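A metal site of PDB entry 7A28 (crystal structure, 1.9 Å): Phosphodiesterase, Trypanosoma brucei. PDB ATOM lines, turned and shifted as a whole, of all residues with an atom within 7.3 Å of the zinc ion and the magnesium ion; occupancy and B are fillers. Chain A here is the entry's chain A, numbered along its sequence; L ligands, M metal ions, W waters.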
ATOM      1  N   TYR A 110     -10.072 -23.085  17.088  1.00  0.00           N
ATOM      2  CA  TYR A 110     -10.974 -23.207  18.267  1.00  0.00           C
ATOM      3  C   TYR A 110     -10.319 -22.676  19.553  1.00  0.00           C
ATOM      4  O   TYR A 110     -10.922 -21.772  20.171  1.00  0.00           O
ATOM      5  CB  TYR A 110     -11.453 -24.646  18.434  1.00  0.00           C
ATOM      6  CG  TYR A 110     -12.463 -24.762  19.558  1.00  0.00           C
ATOM      7  CD1 TYR A 110     -13.793 -24.456  19.357  1.00  0.00           C
ATOM      8  CD2 TYR A 110     -12.085 -25.171  20.830  1.00  0.00           C
ATOM      9  CE1 TYR A 110     -14.738 -24.603  20.365  1.00  0.00           C
ATOM     10  CE2 TYR A 110     -12.998 -25.285  21.860  1.00  0.00           C
ATOM     11  CZ  TYR A 110     -14.334 -24.968  21.638  1.00  0.00           C
ATOM     12  OH  TYR A 110     -15.244 -25.091  22.639  1.00  0.00           O
ATOM     13  N   HIS A 111      -9.146 -23.188  19.948  1.00  0.00           N
ATOM     14  CA  HIS A 111      -8.511 -22.851  21.255  1.00  0.00           C
ATOM     15  C   HIS A 111      -7.723 -21.537  21.130  1.00  0.00           C
ATOM     16  O   HIS A 111      -6.510 -21.518  21.434  1.00  0.00           O
ATOM     17  CB  HIS A 111      -7.664 -24.010  21.772  1.00  0.00           C
ATOM     18  CG  HIS A 111      -8.460 -25.166  22.242  1.00  0.00           C
ATOM     19  ND1 HIS A 111      -8.611 -26.323  21.508  1.00  0.00           N
ATOM     20  CD2 HIS A 111      -9.161 -25.357  23.377  1.00  0.00           C
ATOM     21  CE1 HIS A 111      -9.375 -27.162  22.164  1.00  0.00           C
ATOM     22  NE2 HIS A 111      -9.716 -26.594  23.323  1.00  0.00           N
ATOM     23  N   HIS A 115     -12.401 -18.328  22.356  1.00  0.00           N
ATOM     24  CA  HIS A 115     -12.876 -19.417  23.243  1.00  0.00           C
ATOM     25  C   HIS A 115     -12.802 -18.982  24.722  1.00  0.00           C
ATOM     26  O   HIS A 115     -13.791 -19.219  25.455  1.00  0.00           O
ATOM     27  CB  HIS A 115     -12.089 -20.709  22.988  1.00  0.00           C
ATOM     28  CG  HIS A 115     -12.275 -21.749  24.041  1.00  0.00           C
ATOM     29  ND1 HIS A 115     -13.489 -22.389  24.265  1.00  0.00           N
ATOM     30  CD2 HIS A 115     -11.387 -22.284  24.914  1.00  0.00           C
ATOM     31  CE1 HIS A 115     -13.311 -23.289  25.222  1.00  0.00           C
ATOM     32  NE2 HIS A 115     -12.018 -23.240  25.641  1.00  0.00           N
ATOM     33  N   VAL A 116     -11.714 -18.348  25.179  1.00  0.00           N
ATOM     34  CA  VAL A 116     -11.556 -18.090  26.647  1.00  0.00           C
ATOM     35  C   VAL A 116     -12.445 -16.902  27.031  1.00  0.00           C
ATOM     36  O   VAL A 116     -12.965 -16.914  28.142  1.00  0.00           O
ATOM     37  CB  VAL A 116     -10.086 -17.964  27.090  1.00  0.00           C
ATOM     38  CG1 VAL A 116      -9.265 -19.178  26.660  1.00  0.00           C
ATOM     39  CG2 VAL A 116      -9.392 -16.685  26.652  1.00  0.00           C
ATOM     40  N   VAL A 119     -15.866 -18.477  27.361  1.00  0.00           N
ATOM     41  CA  VAL A 119     -15.974 -19.217  28.658  1.00  0.00           C
ATOM     42  C   VAL A 119     -16.180 -18.220  29.816  1.00  0.00           C
ATOM     43  O   VAL A 119     -17.064 -18.506  30.664  1.00  0.00           O
ATOM     44  CB  VAL A 119     -14.779 -20.150  28.863  1.00  0.00           C
ATOM     45  CG1 VAL A 119     -14.775 -20.730  30.270  1.00  0.00           C
ATOM     46  CG2 VAL A 119     -14.763 -21.273  27.822  1.00  0.00           C
ATOM     47  N   ALA A 148     -11.094 -18.155  33.792  1.00  0.00           N
ATOM     48  CA  ALA A 148     -11.577 -18.383  32.404  1.00  0.00           C
ATOM     49  C   ALA A 148     -10.558 -17.860  31.386  1.00  0.00           C
ATOM     50  O   ALA A 148     -10.314 -18.539  30.342  1.00  0.00           O
ATOM     51  CB  ALA A 148     -12.950 -17.768  32.251  1.00  0.00           C
ATOM     52  N   HIS A 151      -7.216 -20.228  31.152  1.00  0.00           N
ATOM     53  CA  HIS A 151      -7.369 -21.704  31.296  1.00  0.00           C
ATOM     54  C   HIS A 151      -6.806 -22.482  30.076  1.00  0.00           C
ATOM     55  O   HIS A 151      -6.652 -23.709  30.193  1.00  0.00           O
ATOM     56  CB  HIS A 151      -8.817 -22.051  31.665  1.00  0.00           C
ATOM     57  CG  HIS A 151      -9.696 -22.304  30.494  1.00  0.00           C
ATOM     58  ND1 HIS A 151     -10.363 -21.274  29.860  1.00  0.00           N
ATOM     59  CD2 HIS A 151      -9.999 -23.427  29.805  1.00  0.00           C
ATOM     60  CE1 HIS A 151     -11.032 -21.764  28.832  1.00  0.00           C
ATOM     61  NE2 HIS A 151     -10.841 -23.063  28.783  1.00  0.00           N
ATOM     62  N   ASP A 152      -6.528 -21.829  28.935  1.00  0.00           N
ATOM     63  CA  ASP A 152      -5.972 -22.495  27.731  1.00  0.00           C
ATOM     64  C   ASP A 152      -4.717 -21.764  27.180  1.00  0.00           C
ATOM     65  O   ASP A 152      -4.435 -21.964  25.961  1.00  0.00           O
ATOM     66  CB  ASP A 152      -7.069 -22.629  26.654  1.00  0.00           C
ATOM     67  CG  ASP A 152      -7.999 -23.834  26.811  1.00  0.00           C
ATOM     68  OD1 ASP A 152      -7.545 -24.945  27.253  1.00  0.00           O
ATOM     69  OD2 ASP A 152      -9.205 -23.649  26.524  1.00  0.00           O
ATOM     70  N   LEU A 153      -3.974 -21.010  28.003  1.00  0.00           N
ATOM     71  CA  LEU A 153      -2.856 -20.140  27.518  1.00  0.00           C
ATOM     72  C   LEU A 153      -1.887 -20.978  26.672  1.00  0.00           C
ATOM     73  O   LEU A 153      -1.474 -22.060  27.127  1.00  0.00           O
ATOM     74  CB  LEU A 153      -2.087 -19.494  28.686  1.00  0.00           C
ATOM     75  CG  LEU A 153      -2.781 -18.379  29.459  1.00  0.00           C
ATOM     76  CD1 LEU A 153      -2.115 -18.181  30.818  1.00  0.00           C
ATOM     77  CD2 LEU A 153      -2.796 -17.083  28.655  1.00  0.00           C
ATOM     78  N   HIS A 155      -2.237 -22.720  23.950  1.00  0.00           N
ATOM     79  CA  HIS A 155      -2.768 -23.899  23.215  1.00  0.00           C
ATOM     80  C   HIS A 155      -2.338 -23.834  21.736  1.00  0.00           C
ATOM     81  O   HIS A 155      -2.473 -22.751  21.149  1.00  0.00           O
ATOM     82  CB  HIS A 155      -4.315 -23.976  23.335  1.00  0.00           C
ATOM     83  CG  HIS A 155      -4.876 -25.353  23.253  1.00  0.00           C
ATOM     84  ND1 HIS A 155      -4.818 -26.105  22.085  1.00  0.00           N
ATOM     85  CD2 HIS A 155      -5.450 -26.150  24.192  1.00  0.00           C
ATOM     86  CE1 HIS A 155      -5.368 -27.299  22.323  1.00  0.00           C
ATOM     87  NE2 HIS A 155      -5.756 -27.351  23.615  1.00  0.00           N
ATOM     88  N   LEU A 183      -1.125 -30.222  28.778  1.00  0.00           N
ATOM     89  CA  LEU A 183      -1.428 -28.816  28.446  1.00  0.00           C
ATOM     90  C   LEU A 183      -1.842 -28.042  29.714  1.00  0.00           C
ATOM     91  O   LEU A 183      -1.457 -26.851  29.805  1.00  0.00           O
ATOM     92  CB  LEU A 183      -2.505 -28.759  27.370  1.00  0.00           C
ATOM     93  CG  LEU A 183      -1.976 -29.065  25.965  1.00  0.00           C
ATOM     94  CD1 LEU A 183      -3.133 -29.128  24.995  1.00  0.00           C
ATOM     95  CD2 LEU A 183      -0.965 -28.027  25.489  1.00  0.00           C
ATOM     96  N   GLU A 184      -2.581 -28.657  30.619  1.00  0.00           N
ATOM     97  CA  GLU A 184      -3.172 -27.966  31.799  1.00  0.00           C
ATOM     98  C   GLU A 184      -2.049 -27.491  32.710  1.00  0.00           C
ATOM     99  O   GLU A 184      -2.135 -26.362  33.225  1.00  0.00           O
ATOM    100  CB  GLU A 184      -4.206 -28.863  32.516  1.00  0.00           C
ATOM    101  CG  GLU A 184      -5.463 -29.164  31.667  1.00  0.00           C
ATOM    102  CD  GLU A 184      -5.325 -30.182  30.542  1.00  0.00           C
ATOM    103  OE1 GLU A 184      -4.339 -30.930  30.536  1.00  0.00           O
ATOM    104  OE2 GLU A 184      -6.207 -30.205  29.676  1.00  0.00           O
ATOM    105  N   HIS A 187      -0.554 -24.414  30.916  1.00  0.00           N
ATOM    106  CA  HIS A 187      -1.408 -23.215  31.071  1.00  0.00           C
ATOM    107  C   HIS A 187      -1.142 -22.594  32.459  1.00  0.00           C
ATOM    108  O   HIS A 187      -0.984 -21.343  32.541  1.00  0.00           O
ATOM    109  CB  HIS A 187      -2.919 -23.509  30.845  1.00  0.00           C
ATOM    110  CG  HIS A 187      -3.300 -24.299  29.628  1.00  0.00           C
ATOM    111  ND1 HIS A 187      -2.778 -24.053  28.375  1.00  0.00           N
ATOM    112  CD2 HIS A 187      -4.165 -25.328  29.471  1.00  0.00           C
ATOM    113  CE1 HIS A 187      -3.303 -24.888  27.507  1.00  0.00           C
ATOM    114  NE2 HIS A 187      -4.172 -25.678  28.148  1.00  0.00           N
ATOM    115  N   VAL A 222      -8.090 -25.074  36.646  1.00  0.00           N
ATOM    116  CA  VAL A 222      -7.435 -25.322  35.318  1.00  0.00           C
ATOM    117  C   VAL A 222      -7.062 -26.800  35.198  1.00  0.00           C
ATOM    118  O   VAL A 222      -7.295 -27.370  34.168  1.00  0.00           O
ATOM    119  CB  VAL A 222      -6.211 -24.414  35.115  1.00  0.00           C
ATOM    120  CG1 VAL A 222      -5.466 -24.765  33.850  1.00  0.00           C
ATOM    121  CG2 VAL A 222      -6.581 -22.953  35.164  1.00  0.00           C
ATOM    122  N   THR A 225      -9.963 -29.179  34.122  1.00  0.00           N
ATOM    123  CA  THR A 225     -10.494 -29.108  32.712  1.00  0.00           C
ATOM    124  C   THR A 225      -9.952 -30.262  31.838  1.00  0.00           C
ATOM    125  O   THR A 225     -10.441 -30.376  30.682  1.00  0.00           O
ATOM    126  CB  THR A 225     -10.199 -27.763  32.021  1.00  0.00           C
ATOM    127  OG1 THR A 225      -8.797 -27.475  31.921  1.00  0.00           O
ATOM    128  CG2 THR A 225     -10.859 -26.599  32.713  1.00  0.00           C
ATOM    129  N   ASP A 226      -8.992 -31.074  32.319  1.00  0.00           N
ATOM    130  CA  ASP A 226      -8.499 -32.272  31.583  1.00  0.00           C
ATOM    131  C   ASP A 226      -9.644 -33.291  31.464  1.00  0.00           C
ATOM    132  O   ASP A 226     -10.089 -33.873  32.478  1.00  0.00           O
ATOM    133  CB  ASP A 226      -7.240 -32.856  32.234  1.00  0.00           C
ATOM    134  CG  ASP A 226      -6.669 -34.131  31.597  1.00  0.00           C
ATOM    135  OD1 ASP A 226      -7.277 -34.655  30.662  1.00  0.00           O
ATOM    136  OD2 ASP A 226      -5.594 -34.548  32.046  1.00  0.00           O
ATOM    137  N   LEU A 260     -16.167 -24.054  35.913  1.00  0.00           N
ATOM    138  CA  LEU A 260     -15.192 -23.904  34.807  1.00  0.00           C
ATOM    139  C   LEU A 260     -15.374 -25.059  33.799  1.00  0.00           C
ATOM    140  O   LEU A 260     -15.380 -24.771  32.623  1.00  0.00           O
ATOM    141  CB  LEU A 260     -13.747 -23.859  35.301  1.00  0.00           C
ATOM    142  CG  LEU A 260     -12.699 -23.733  34.198  1.00  0.00           C
ATOM    143  CD1 LEU A 260     -12.885 -22.489  33.339  1.00  0.00           C
ATOM    144  CD2 LEU A 260     -11.305 -23.725  34.760  1.00  0.00           C
ATOM    145  N   GLY A 263     -18.542 -24.251  31.697  1.00  0.00           N
ATOM    146  CA  GLY A 263     -18.245 -23.213  30.691  1.00  0.00           C
ATOM    147  C   GLY A 263     -17.486 -23.820  29.523  1.00  0.00           C
ATOM    148  O   GLY A 263     -17.790 -23.505  28.337  1.00  0.00           O
ATOM    149  N   ASP A 264     -16.529 -24.685  29.807  1.00  0.00           N
ATOM    150  CA  ASP A 264     -15.671 -25.304  28.774  1.00  0.00           C
ATOM    151  C   ASP A 264     -16.475 -26.200  27.811  1.00  0.00           C
ATOM    152  O   ASP A 264     -16.081 -26.297  26.654  1.00  0.00           O
ATOM    153  CB  ASP A 264     -14.511 -26.047  29.420  1.00  0.00           C
ATOM    154  CG  ASP A 264     -13.249 -26.062  28.584  1.00  0.00           C
ATOM    155  OD1 ASP A 264     -13.051 -25.092  27.806  1.00  0.00           O
ATOM    156  OD2 ASP A 264     -12.475 -27.012  28.737  1.00  0.00           O
ATOM    157  N   ILE A 265     -17.557 -26.868  28.236  1.00  0.00           N
ATOM    158  CA  ILE A 265     -18.415 -27.715  27.344  1.00  0.00           C
ATOM    159  C   ILE A 265     -19.819 -27.086  27.174  1.00  0.00           C
ATOM    160  O   ILE A 265     -20.799 -27.837  26.928  1.00  0.00           O
ATOM    161  CB  ILE A 265     -18.451 -29.178  27.835  1.00  0.00           C
ATOM    162  CG1 ILE A 265     -19.089 -29.329  29.209  1.00  0.00           C
ATOM    163  CG2 ILE A 265     -17.052 -29.806  27.840  1.00  0.00           C
ATOM    164  CD1 ILE A 265     -19.395 -30.761  29.541  1.00  0.00           C
HETATM  165  C1  LIG L   1     -13.731 -30.815  23.758  1.00  0.00           C
HETATM  166  C2  LIG L   1     -12.821 -29.788  23.069  1.00  0.00           C
HETATM  167  C3  LIG L   1     -14.361 -30.225  25.021  1.00  0.00           C
HETATM  168  C4  LIG L   1     -14.783 -31.386  22.804  1.00  0.00           C
HETATM  169  C5  LIG L   1     -15.809 -30.699  22.017  1.00  0.00           C
HETATM  170  C6  LIG L   1     -16.216 -29.404  22.310  1.00  0.00           C
HETATM  171  C7  LIG L   1     -17.236 -28.812  21.592  1.00  0.00           C
HETATM  172  C8  LIG L   1     -17.848 -29.511  20.559  1.00  0.00           C
HETATM  173  C9  LIG L   1     -19.128 -27.658  19.824  1.00  0.00           C
HETATM  174  C10 LIG L   1     -17.721 -33.417  17.922  1.00  0.00           C
HETATM  175  C11 LIG L   1     -17.953 -34.901  17.914  1.00  0.00           C
HETATM  176  C12 LIG L   1     -17.723 -35.460  19.269  1.00  0.00           C
HETATM  177  C13 LIG L   1     -19.211 -38.520  20.200  1.00  0.00           C
HETATM  178  C14 LIG L   1     -18.739 -39.329  22.404  1.00  0.00           C
HETATM  179  C15 LIG L   1     -17.810 -37.251  21.650  1.00  0.00           C
HETATM  180  C16 LIG L   1     -16.422 -31.381  20.969  1.00  0.00           C
HETATM  181  C17 LIG L   1     -13.524 -34.493  23.514  1.00  0.00           C
HETATM  182  C18 LIG L   1     -12.465 -35.035  22.602  1.00  0.00           C
HETATM  183  C19 LIG L   1     -12.552 -36.533  22.335  1.00  0.00           C
HETATM  184  C20 LIG L   1     -13.883 -37.167  22.663  1.00  0.00           C
HETATM  185  C21 LIG L   1     -13.648 -35.060  24.862  1.00  0.00           C
HETATM  186  N1  LIG L   1     -19.412 -41.578  23.211  1.00  0.00           N
HETATM  187  C22 LIG L   1     -12.995 -32.079  24.113  1.00  0.00           C
HETATM  188  O1  LIG L   1     -12.007 -32.200  24.798  1.00  0.00           O
HETATM  189  C23 LIG L   1     -17.418 -30.791  20.247  1.00  0.00           C
HETATM  190  C24 LIG L   1     -18.046 -32.839  19.257  1.00  0.00           C
HETATM  191  C25 LIG L   1     -18.433 -37.420  20.440  1.00  0.00           C
HETATM  192  C26 LIG L   1     -19.373 -39.462  21.187  1.00  0.00           C
HETATM  193  C27 LIG L   1     -18.825 -40.412  23.385  1.00  0.00           C
HETATM  194  C28 LIG L   1     -17.962 -38.212  22.628  1.00  0.00           C
HETATM  195  C29 LIG L   1     -14.225 -37.433  24.117  1.00  0.00           C
HETATM  196  C30 LIG L   1     -14.588 -36.239  24.968  1.00  0.00           C
HETATM  197  N2  LIG L   1     -19.251 -42.265  24.368  1.00  0.00           N
HETATM  198  N3  LIG L   1     -18.575 -41.561  25.219  1.00  0.00           N
HETATM  199  N4  LIG L   1     -18.286 -40.403  24.610  1.00  0.00           N
HETATM  200  N5  LIG L   1     -14.713 -32.636  22.721  1.00  0.00           N
HETATM  201  N6  LIG L   1     -13.710 -33.042  23.497  1.00  0.00           N
HETATM  202  O2  LIG L   1     -18.898 -29.044  19.837  1.00  0.00           O
HETATM  203  O3  LIG L   1     -18.002 -31.424  19.191  1.00  0.00           O
HETATM  204  O4  LIG L   1     -18.430 -36.683  19.297  1.00  0.00           O
HETATM  205 ZN    ZN M   1     -11.098 -24.534  27.107  1.00  0.00          ZN
HETATM  206 MG    MG M   2      -8.093 -26.799  27.883  1.00  0.00          MG
HETATM  207  O   HOH W   1     -10.016 -26.129  27.868  1.00  0.00           O
HETATM  208  O   HOH W   2      -7.386 -26.283  30.059  1.00  0.00           O
HETATM  209  O   HOH W   3      -5.942 -27.558  27.314  1.00  0.00           O
HETATM  210  O   HOH W   4      -8.442 -28.874  29.124  1.00  0.00           O
HETATM  211  O   HOH W   5      -8.819 -27.970  25.882  1.00  0.00           O
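O of Ala 148 is in hydrogen-bond range of ND1 of His 151.
Of the 20 residues printed, 4 come within 4 Å of the zinc ion.
One residue has an atom within 4 Å of the magnesium ion: Asp 152. The nearest printed residue that does not touch the magnesium ion is His 187 (4.1 Å).
The zinc ion is bound by water W1 (2.1 Å), OD1 of Asp 264 (2.1 Å), NE2 of His 115 (2.2 Å), OD2 of Asp 152 (2.2 Å) and NE2 of His 151 (2.2 Å). The zinc ion has five donor atoms within binding distance.
The magnesium ion is bound by OD1 of Asp 152 (2.0 Å), water W1 (2.0 Å), water W2 (2.3 Å), water W3 (2.4 Å), water W5 (2.4 Å) and water W4 (2.4 Å). The magnesium ion has six donor atoms within binding distance.
Water W2 bridges OG1 of Thr 225 (2.6 Å) and O of His 151 (2.7 Å). Water W4 bridges the side-chain carboxylate of Glu 184 (2.7 Å) and the backbone carbonyl oxygen of Thr 225 (2.9 Å).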
